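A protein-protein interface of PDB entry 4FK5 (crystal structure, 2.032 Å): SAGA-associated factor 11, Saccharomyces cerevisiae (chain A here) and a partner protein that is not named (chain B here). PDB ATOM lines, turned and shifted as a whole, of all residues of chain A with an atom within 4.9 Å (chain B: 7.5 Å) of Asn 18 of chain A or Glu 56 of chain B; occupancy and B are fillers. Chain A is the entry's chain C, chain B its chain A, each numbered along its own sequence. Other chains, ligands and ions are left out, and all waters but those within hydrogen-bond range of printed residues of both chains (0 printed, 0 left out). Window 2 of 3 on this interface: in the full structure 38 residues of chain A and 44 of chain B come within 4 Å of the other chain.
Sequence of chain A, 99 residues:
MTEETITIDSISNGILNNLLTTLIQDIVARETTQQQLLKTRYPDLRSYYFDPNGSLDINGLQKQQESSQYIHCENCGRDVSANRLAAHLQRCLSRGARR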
ATOM      1  N   GLY A  14      -0.254  -2.049 -33.414  1.00  0.00           N
ATOM      2  CA  GLY A  14       0.258  -2.290 -32.018  1.00  0.00           C
ATOM      3  C   GLY A  14       1.514  -1.422 -31.745  1.00  0.00           C
ATOM      4  O   GLY A  14       1.621  -0.774 -30.709  1.00  0.00           O
ATOM      5  N   ILE A  15       2.428  -1.389 -32.696  1.00  0.00           N
ATOM      6  CA  ILE A  15       3.668  -0.572 -32.557  1.00  0.00           C
ATOM      7  C   ILE A  15       3.361   0.928 -32.414  1.00  0.00           C
ATOM      8  O   ILE A  15       3.846   1.571 -31.486  1.00  0.00           O
ATOM      9  CB  ILE A  15       4.699  -0.886 -33.684  1.00  0.00           C
ATOM     10  CG1 ILE A  15       5.236  -2.303 -33.487  1.00  0.00           C
ATOM     11  CG2 ILE A  15       5.869   0.124 -33.702  1.00  0.00           C
ATOM     12  CD1 ILE A  15       5.877  -2.924 -34.708  1.00  0.00           C
ATOM     13  N   LEU A  16       2.445   1.446 -33.238  1.00  0.00           N
ATOM     14  CA  LEU A  16       2.049   2.818 -33.159  1.00  0.00           C
ATOM     15  C   LEU A  16       1.375   3.108 -31.856  1.00  0.00           C
ATOM     16  O   LEU A  16       1.651   4.138 -31.234  1.00  0.00           O
ATOM     17  CB  LEU A  16       1.122   3.209 -34.333  1.00  0.00           C
ATOM     18  CG  LEU A  16       0.705   4.669 -34.400  1.00  0.00           C
ATOM     19  CD1 LEU A  16       1.899   5.593 -34.402  1.00  0.00           C
ATOM     20  CD2 LEU A  16      -0.182   4.918 -35.603  1.00  0.00           C
ATOM     21  N   ASN A  17       0.507   2.185 -31.404  1.00  0.00           N
ATOM     22  CA  ASN A  17      -0.172   2.382 -30.150  1.00  0.00           C
ATOM     23  C   ASN A  17       0.810   2.392 -28.963  1.00  0.00           C
ATOM     24  O   ASN A  17       0.651   3.181 -28.037  1.00  0.00           O
ATOM     25  CB  ASN A  17      -1.263   1.346 -29.934  1.00  0.00           C
ATOM     26  CG  ASN A  17      -2.114   1.626 -28.673  1.00  0.00           C
ATOM     27  OD1 ASN A  17      -1.968   0.936 -27.666  1.00  0.00           O
ATOM     28  ND2 ASN A  17      -2.980   2.615 -28.733  1.00  0.00           N
ATOM     29  N   ASN A  18       1.836   1.554 -29.013  1.00  0.00           N
ATOM     30  CA  ASN A  18       2.917   1.673 -28.018  1.00  0.00           C
ATOM     31  C   ASN A  18       3.534   3.073 -28.032  1.00  0.00           C
ATOM     32  O   ASN A  18       3.562   3.760 -27.025  1.00  0.00           O
ATOM     33  CB  ASN A  18       3.959   0.533 -28.166  1.00  0.00           C
ATOM     34  CG  ASN A  18       3.503  -0.800 -27.475  1.00  0.00           C
ATOM     35  OD1 ASN A  18       4.344  -1.632 -27.024  1.00  0.00           O
ATOM     36  ND2 ASN A  18       2.249  -1.033 -27.467  1.00  0.00           N
ATOM     37  N   LEU A  19       3.945   3.542 -29.197  1.00  0.00           N
ATOM     38  CA  LEU A  19       4.562   4.857 -29.265  1.00  0.00           C
ATOM     39  C   LEU A  19       3.632   5.951 -28.771  1.00  0.00           C
ATOM     40  O   LEU A  19       4.058   6.815 -28.009  1.00  0.00           O
ATOM     41  CB  LEU A  19       5.010   5.162 -30.662  1.00  0.00           C
ATOM     42  CG  LEU A  19       6.159   4.308 -31.192  1.00  0.00           C
ATOM     43  CD1 LEU A  19       6.154   4.331 -32.719  1.00  0.00           C
ATOM     44  CD2 LEU A  19       7.507   4.821 -30.647  1.00  0.00           C
ATOM     45  N   LEU A  20       2.365   5.941 -29.218  1.00  0.00           N
ATOM     46  CA  LEU A  20       1.439   6.989 -28.864  1.00  0.00           C
ATOM     47  C   LEU A  20       1.062   7.005 -27.363  1.00  0.00           C
ATOM     48  O   LEU A  20       1.120   8.050 -26.752  1.00  0.00           O
ATOM     49  CB  LEU A  20       0.135   6.899 -29.691  1.00  0.00           C
ATOM     50  CG  LEU A  20       0.292   7.333 -31.164  1.00  0.00           C
ATOM     51  CD1 LEU A  20      -1.062   6.998 -31.941  1.00  0.00           C
ATOM     52  CD2 LEU A  20       0.659   8.779 -31.199  1.00  0.00           C
ATOM     53  N   THR A  21       0.681   5.856 -26.802  1.00  0.00           N
ATOM     54  CA  THR A  21       0.277   5.828 -25.361  1.00  0.00           C
ATOM     55  C   THR A  21       1.461   6.217 -24.462  1.00  0.00           C
ATOM     56  O   THR A  21       1.285   6.950 -23.505  1.00  0.00           O
ATOM     57  CB  THR A  21      -0.261   4.464 -24.885  1.00  0.00           C
ATOM     58  OG1 THR A  21       0.710   3.467 -25.121  1.00  0.00           O
ATOM     59  CG2 THR A  21      -1.662   4.048 -25.639  1.00  0.00           C
ATOM     60  N   THR A  22       2.669   5.782 -24.825  1.00  0.00           N
ATOM     61  CA  THR A  22       3.859   6.233 -24.108  1.00  0.00           C
ATOM     62  C   THR A  22       4.003   7.706 -24.080  1.00  0.00           C
ATOM     63  O   THR A  22       4.238   8.306 -23.009  1.00  0.00           O
ATOM     64  CB  THR A  22       5.161   5.545 -24.622  1.00  0.00           C
ATOM     65  OG1 THR A  22       5.020   4.145 -24.490  1.00  0.00           O
ATOM     66  CG2 THR A  22       6.391   6.022 -23.801  1.00  0.00           C
ATOM     67  N   PHE B  45      16.267   2.641 -25.008  1.00  0.00           N
ATOM     68  CA  PHE B  45      15.107   1.791 -25.383  1.00  0.00           C
ATOM     69  C   PHE B  45      15.258   0.377 -24.787  1.00  0.00           C
ATOM     70  O   PHE B  45      14.332  -0.137 -24.208  1.00  0.00           O
ATOM     71  CB  PHE B  45      14.875   1.720 -26.909  1.00  0.00           C
ATOM     72  CG  PHE B  45      14.374   3.015 -27.523  1.00  0.00           C
ATOM     73  CD1 PHE B  45      13.171   3.552 -27.163  1.00  0.00           C
ATOM     74  CD2 PHE B  45      15.060   3.611 -28.551  1.00  0.00           C
ATOM     75  CE1 PHE B  45      12.720   4.755 -27.759  1.00  0.00           C
ATOM     76  CE2 PHE B  45      14.591   4.773 -29.156  1.00  0.00           C
ATOM     77  CZ  PHE B  45      13.428   5.343 -28.740  1.00  0.00           C
ATOM     78  N   MET B  49      13.286   1.096 -21.271  1.00  0.00           N
ATOM     79  CA  MET B  49      11.947   1.135 -21.842  1.00  0.00           C
ATOM     80  C   MET B  49      11.449  -0.218 -22.320  1.00  0.00           C
ATOM     81  O   MET B  49      10.504  -0.292 -23.087  1.00  0.00           O
ATOM     82  CB  MET B  49      11.918   2.145 -23.002  1.00  0.00           C
ATOM     83  CG  MET B  49      12.049   3.555 -22.485  1.00  0.00           C
ATOM     84  SD  MET B  49      12.236   4.789 -23.765  1.00  0.00           S
ATOM     85  CE  MET B  49      12.435   6.226 -22.639  1.00  0.00           C
ATOM     86  N   LYS B  50      12.065  -1.276 -21.801  1.00  0.00           N
ATOM     87  CA  LYS B  50      11.710  -2.655 -22.182  1.00  0.00           C
ATOM     88  C   LYS B  50      11.162  -3.344 -20.939  1.00  0.00           C
ATOM     89  O   LYS B  50      11.822  -3.386 -19.912  1.00  0.00           O
ATOM     90  CB  LYS B  50      12.931  -3.407 -22.674  1.00  0.00           C
ATOM     91  CG  LYS B  50      12.623  -4.876 -23.048  1.00  0.00           C
ATOM     92  CD  LYS B  50      13.891  -5.676 -23.219  1.00  0.00           C
ATOM     93  CE  LYS B  50      13.871  -6.506 -24.498  1.00  0.00           C
ATOM     94  NZ  LYS B  50      14.493  -7.858 -24.280  1.00  0.00           N
ATOM     95  N   CYS B  51       9.935  -3.823 -21.009  1.00  0.00           N
ATOM     96  CA  CYS B  51       9.299  -4.413 -19.828  1.00  0.00           C
ATOM     97  C   CYS B  51       9.974  -5.754 -19.487  1.00  0.00           C
ATOM     98  O   CYS B  51      10.103  -6.622 -20.334  1.00  0.00           O
ATOM     99  CB  CYS B  51       7.811  -4.628 -20.083  1.00  0.00           C
ATOM    100  SG  CYS B  51       6.961  -5.333 -18.618  1.00  0.00           S
ATOM    101  N   GLY B  52      10.379  -5.925 -18.255  1.00  0.00           N
ATOM    102  CA  GLY B  52      10.972  -7.229 -17.852  1.00  0.00           C
ATOM    103  C   GLY B  52      10.001  -8.458 -17.883  1.00  0.00           C
ATOM    104  O   GLY B  52      10.445  -9.568 -17.909  1.00  0.00           O
ATOM    105  N   THR B  53       8.693  -8.213 -17.891  1.00  0.00           N
ATOM    106  CA  THR B  53       7.698  -9.284 -17.907  1.00  0.00           C
ATOM    107  C   THR B  53       7.288  -9.610 -19.355  1.00  0.00           C
ATOM    108  O   THR B  53       7.498 -10.709 -19.787  1.00  0.00           O
ATOM    109  CB  THR B  53       6.489  -8.908 -17.071  1.00  0.00           C
ATOM    110  OG1 THR B  53       6.922  -8.551 -15.762  1.00  0.00           O
ATOM    111  CG2 THR B  53       5.482 -10.095 -16.957  1.00  0.00           C
ATOM    112  N   CYS B  54       6.783  -8.631 -20.126  1.00  0.00           N
ATOM    113  CA  CYS B  54       6.357  -8.904 -21.527  1.00  0.00           C
ATOM    114  C   CYS B  54       7.443  -8.636 -22.565  1.00  0.00           C
ATOM    115  O   CYS B  54       7.254  -8.937 -23.744  1.00  0.00           O
ATOM    116  CB  CYS B  54       5.068  -8.111 -21.902  1.00  0.00           C
ATOM    117  SG  CYS B  54       5.175  -6.253 -21.726  1.00  0.00           S
ATOM    118  N   HIS B  55       8.544  -7.971 -22.164  1.00  0.00           N
ATOM    119  CA  HIS B  55       9.651  -7.647 -23.118  1.00  0.00           C
ATOM    120  C   HIS B  55       9.286  -6.645 -24.260  1.00  0.00           C
ATOM    121  O   HIS B  55      10.020  -6.508 -25.231  1.00  0.00           O
ATOM    122  CB  HIS B  55      10.233  -8.949 -23.715  1.00  0.00           C
ATOM    123  CG  HIS B  55      10.435 -10.023 -22.703  1.00  0.00           C
ATOM    124  ND1 HIS B  55      11.308  -9.899 -21.670  1.00  0.00           N
ATOM    125  CD2 HIS B  55       9.813 -11.277 -22.547  1.00  0.00           C
ATOM    126  CE1 HIS B  55      11.271 -11.001 -20.917  1.00  0.00           C
ATOM    127  NE2 HIS B  55      10.339 -11.843 -21.439  1.00  0.00           N
ATOM    128  N   GLU B  56       8.130  -6.015 -24.176  1.00  0.00           N
ATOM    129  CA  GLU B  56       7.761  -4.992 -25.151  1.00  0.00           C
ATOM    130  C   GLU B  56       8.521  -3.696 -24.872  1.00  0.00           C
ATOM    131  O   GLU B  56       8.783  -3.341 -23.716  1.00  0.00           O
ATOM    132  CB  GLU B  56       6.278  -4.700 -25.097  1.00  0.00           C
ATOM    133  CG  GLU B  56       5.412  -5.658 -25.897  1.00  0.00           C
ATOM    134  CD  GLU B  56       3.916  -5.275 -25.866  1.00  0.00           C
ATOM    135  OE1 GLU B  56       3.065  -6.197 -25.705  1.00  0.00           O
ATOM    136  OE2 GLU B  56       3.572  -4.076 -26.053  1.00  0.00           O
ATOM    137  N   ILE B  57       8.763  -2.956 -25.929  1.00  0.00           N
ATOM    138  CA  ILE B  57       9.348  -1.634 -25.837  1.00  0.00           C
ATOM    139  C   ILE B  57       8.180  -0.661 -25.768  1.00  0.00           C
ATOM    140  O   ILE B  57       7.278  -0.730 -26.598  1.00  0.00           O
ATOM    141  CB  ILE B  57      10.202  -1.316 -27.089  1.00  0.00           C
ATOM    142  CG1 ILE B  57      11.262  -2.434 -27.372  1.00  0.00           C
ATOM    143  CG2 ILE B  57      10.978   0.041 -26.913  1.00  0.00           C
ATOM    144  CD1 ILE B  57      12.213  -2.648 -26.191  1.00  0.00           C
ATOM    145  N   ASN B  58       8.230   0.289 -24.852  1.00  0.00           N
ATOM    146  CA  ASN B  58       7.236   1.388 -24.843  1.00  0.00           C
ATOM    147  C   ASN B  58       5.780   0.846 -24.744  1.00  0.00           C
ATOM    148  O   ASN B  58       4.895   1.285 -25.485  1.00  0.00           O
ATOM    149  CB  ASN B  58       7.324   2.243 -26.099  1.00  0.00           C
ATOM    150  CG  ASN B  58       8.594   3.119 -26.179  1.00  0.00           C
ATOM    151  OD1 ASN B  58       9.076   3.410 -27.300  1.00  0.00           O
ATOM    152  ND2 ASN B  58       9.132   3.522 -25.046  1.00  0.00           N
ATOM    153  N   SER B  59       5.564  -0.123 -23.884  1.00  0.00           N
ATOM    154  CA  SER B  59       4.182  -0.608 -23.530  1.00  0.00           C
ATOM    155  C   SER B  59       3.564   0.369 -22.531  1.00  0.00           C
ATOM    156  O   SER B  59       3.408   0.071 -21.331  1.00  0.00           O
ATOM    157  CB  SER B  59       4.271  -2.030 -22.938  1.00  0.00           C
ATOM    158  OG  SER B  59       2.999  -2.615 -22.683  1.00  0.00           O
ATOM    159  N   GLY B  60       3.243   1.550 -23.021  1.00  0.00           N
ATOM    160  CA  GLY B  60       3.138   2.722 -22.200  1.00  0.00           C
ATOM    161  C   GLY B  60       4.437   3.082 -21.534  1.00  0.00           C
ATOM    162  O   GLY B  60       5.459   2.521 -21.858  1.00  0.00           O
ATOM    163  N   ALA B  61       4.387   4.023 -20.577  1.00  0.00           N
ATOM    164  CA  ALA B  61       5.496   4.263 -19.685  1.00  0.00           C
ATOM    165  C   ALA B  61       6.100   2.950 -19.159  1.00  0.00           C
ATOM    166  O   ALA B  61       5.348   1.972 -18.761  1.00  0.00           O
ATOM    167  CB  ALA B  61       5.057   5.177 -18.493  1.00  0.00           C
ATOM    168  N   THR B  62       7.430   2.951 -19.029  1.00  0.00           N
ATOM    169  CA  THR B  62       8.163   1.900 -18.363  1.00  0.00           C
ATOM    170  C   THR B  62       8.783   2.502 -17.099  1.00  0.00           C
ATOM    171  O   THR B  62       9.346   3.651 -17.097  1.00  0.00           O
ATOM    172  CB  THR B  62       9.204   1.259 -19.320  1.00  0.00           C
ATOM    173  OG1 THR B  62       8.543   0.809 -20.537  1.00  0.00           O
ATOM    174  CG2 THR B  62       9.902   0.093 -18.713  1.00  0.00           C
ATOM    175  N   CYS B  73       6.196  -2.329 -17.428  1.00  0.00           N
ATOM    176  CA  CYS B  73       5.298  -1.441 -18.222  1.00  0.00           C
ATOM    177  C   CYS B  73       4.019  -1.025 -17.488  1.00  0.00           C
ATOM    178  O   CYS B  73       3.575  -1.661 -16.511  1.00  0.00           O
ATOM    179  CB  CYS B  73       4.919  -2.069 -19.550  1.00  0.00           C
ATOM    180  SG  CYS B  73       3.767  -3.533 -19.431  1.00  0.00           S
ATOM    181  N   ASN B  75       1.100  -0.478 -19.637  1.00  0.00           N
ATOM    182  CA  ASN B  75      -0.125  -0.829 -20.378  1.00  0.00           C
ATOM    183  C   ASN B  75      -0.660  -2.225 -20.029  1.00  0.00           C
ATOM    184  O   ASN B  75      -1.856  -2.431 -20.078  1.00  0.00           O
ATOM    185  CB  ASN B  75       0.052  -0.711 -21.893  1.00  0.00           C
ATOM    186  CG  ASN B  75       0.023   0.716 -22.385  1.00  0.00           C
ATOM    187  OD1 ASN B  75       0.054   0.966 -23.589  1.00  0.00           O
ATOM    188  ND2 ASN B  75      -0.043   1.620 -21.504  1.00  0.00           N
ATOM    189  N   HIS B  76       0.223  -3.158 -19.682  1.00  0.00           N
ATOM    190  CA  HIS B  76      -0.200  -4.496 -19.214  1.00  0.00           C
ATOM    191  C   HIS B  76      -0.102  -4.608 -17.722  1.00  0.00           C
ATOM    192  O   HIS B  76      -0.020  -5.703 -17.188  1.00  0.00           O
ATOM    193  CB  HIS B  76       0.650  -5.578 -19.872  1.00  0.00           C
ATOM    194  CG  HIS B  76       0.578  -5.573 -21.364  1.00  0.00           C
ATOM    195  ND1 HIS B  76      -0.598  -5.512 -22.037  1.00  0.00           N
ATOM    196  CD2 HIS B  76       1.591  -5.608 -22.336  1.00  0.00           C
ATOM    197  CE1 HIS B  76      -0.352  -5.501 -23.363  1.00  0.00           C
ATOM    198  NE2 HIS B  76       0.993  -5.564 -23.545  1.00  0.00           N
ATOM    199  N   HIS B  78       2.379  -4.287 -15.663  1.00  0.00           N
ATOM    200  CA  HIS B  78       3.377  -5.153 -15.145  1.00  0.00           C
ATOM    201  C   HIS B  78       4.189  -4.616 -13.998  1.00  0.00           C
ATOM    202  O   HIS B  78       4.695  -5.401 -13.183  1.00  0.00           O
ATOM    203  CB  HIS B  78       4.240  -5.708 -16.227  1.00  0.00           C
ATOM    204  CG  HIS B  78       3.547  -6.730 -17.068  1.00  0.00           C
ATOM    205  ND1 HIS B  78       3.710  -6.803 -18.401  1.00  0.00           N
ATOM    206  CD2 HIS B  78       2.640  -7.791 -16.709  1.00  0.00           C
ATOM    207  CE1 HIS B  78       2.965  -7.817 -18.899  1.00  0.00           C
ATOM    208  NE2 HIS B  78       2.321  -8.437 -17.848  1.00  0.00           N
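The side-chain carboxylate of Glu 56 of chain B lies close to the side-chain amide oxygen of Asn 18 of chain A, at 2.7 Å.
O of Asn 58 of chain B lies within hydrogen-bond range of OG1 of Thr 22 of chain A, at 3.0 Å.
The side-chain amide oxygen (OD1) of Asn 75 of chain B lies within hydrogen-bond range of the side-chain hydroxyl (OG1) of Thr 21 of chain A.
O of Gly 60 of chain B sits at hydrogen-bond distance from OG1 of Thr 22 of chain A (3.1 Å).
The backbone carbonyl oxygen (O) of Asn 58 of chain B lies close to the side-chain amide oxygen (OD1) of Asn 18 of chain A, at 3.3 Å.
The backbone carbonyl oxygen of Ile 57 of chain B lies close to the side-chain amide oxygen of Asn 18 of chain A (3.1 Å).
The side-chain amide oxygen of Asn 75 of chain B lies within hydrogen-bond range of the backbone NH of Gly 60 of chain B (3.3 Å).
O of Ser 59 of chain B lies within hydrogen-bond range of N of Asn 75 of chain B, at 2.9 Å.
The backbone carbonyl oxygen of Asn 18 of chain A lies within hydrogen-bond range of the side-chain hydroxyl of Thr 21 of chain A (3.4 Å).
O of Gly 14 of chain A is in hydrogen-bond range of ND2 of Asn 18 of chain A (3.3 Å).
OG1 of Thr 21 of chain A sits at hydrogen-bond distance from O of Asn 17 of chain A.
O of Asn 18 of chain A is in hydrogen-bond range of OG1 of Thr 22 of chain A (2.9 Å).
Asn 18 of chain A touches Ser 59 of chain B.
Leu 19 of chain A touches Asn 58 of chain B (CD2 to OD1, 3.96 Å).
Gly 60 of chain B touches Thr 21 of chain A.
Thr 22 of chain A touches Ala 61 of chain B (OG1 to N, 3.97 Å).
Glu 56 of chain B touches one residue of chain A.
Printed residues of chain A within 4 Å of Asn 58 of chain B: Asn 18, Leu 19 and Thr 22.
Of the printed residues of chain B, Leu 19 of chain A touches Asn 58.
Asn 17 of chain A touches none of the printed residues of chain B.
Thr 62 of chain B touches none of the printed residues of chain A.
The nearest printed residue of chain A that does not touch Glu 56 of chain B is Gly 14 of chain A (6.0 Å).
The nearest printed residue of chain A that does not touch Asn 75 of chain B is Asn 17 of chain A (4.6 Å).
Printed residues of chain B that touch a printed residue of chain A: Glu 56, Ile 57, Asn 58, Ser 59, Gly 60, Ala 61 and Asn 75.
Among the printed residues, 10 pairs touch across the chains.
Among the printed residues, no Asp or Glu carboxylate lies within 4 Å of a Lys or Arg side-chain nitrogen of the other chain.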
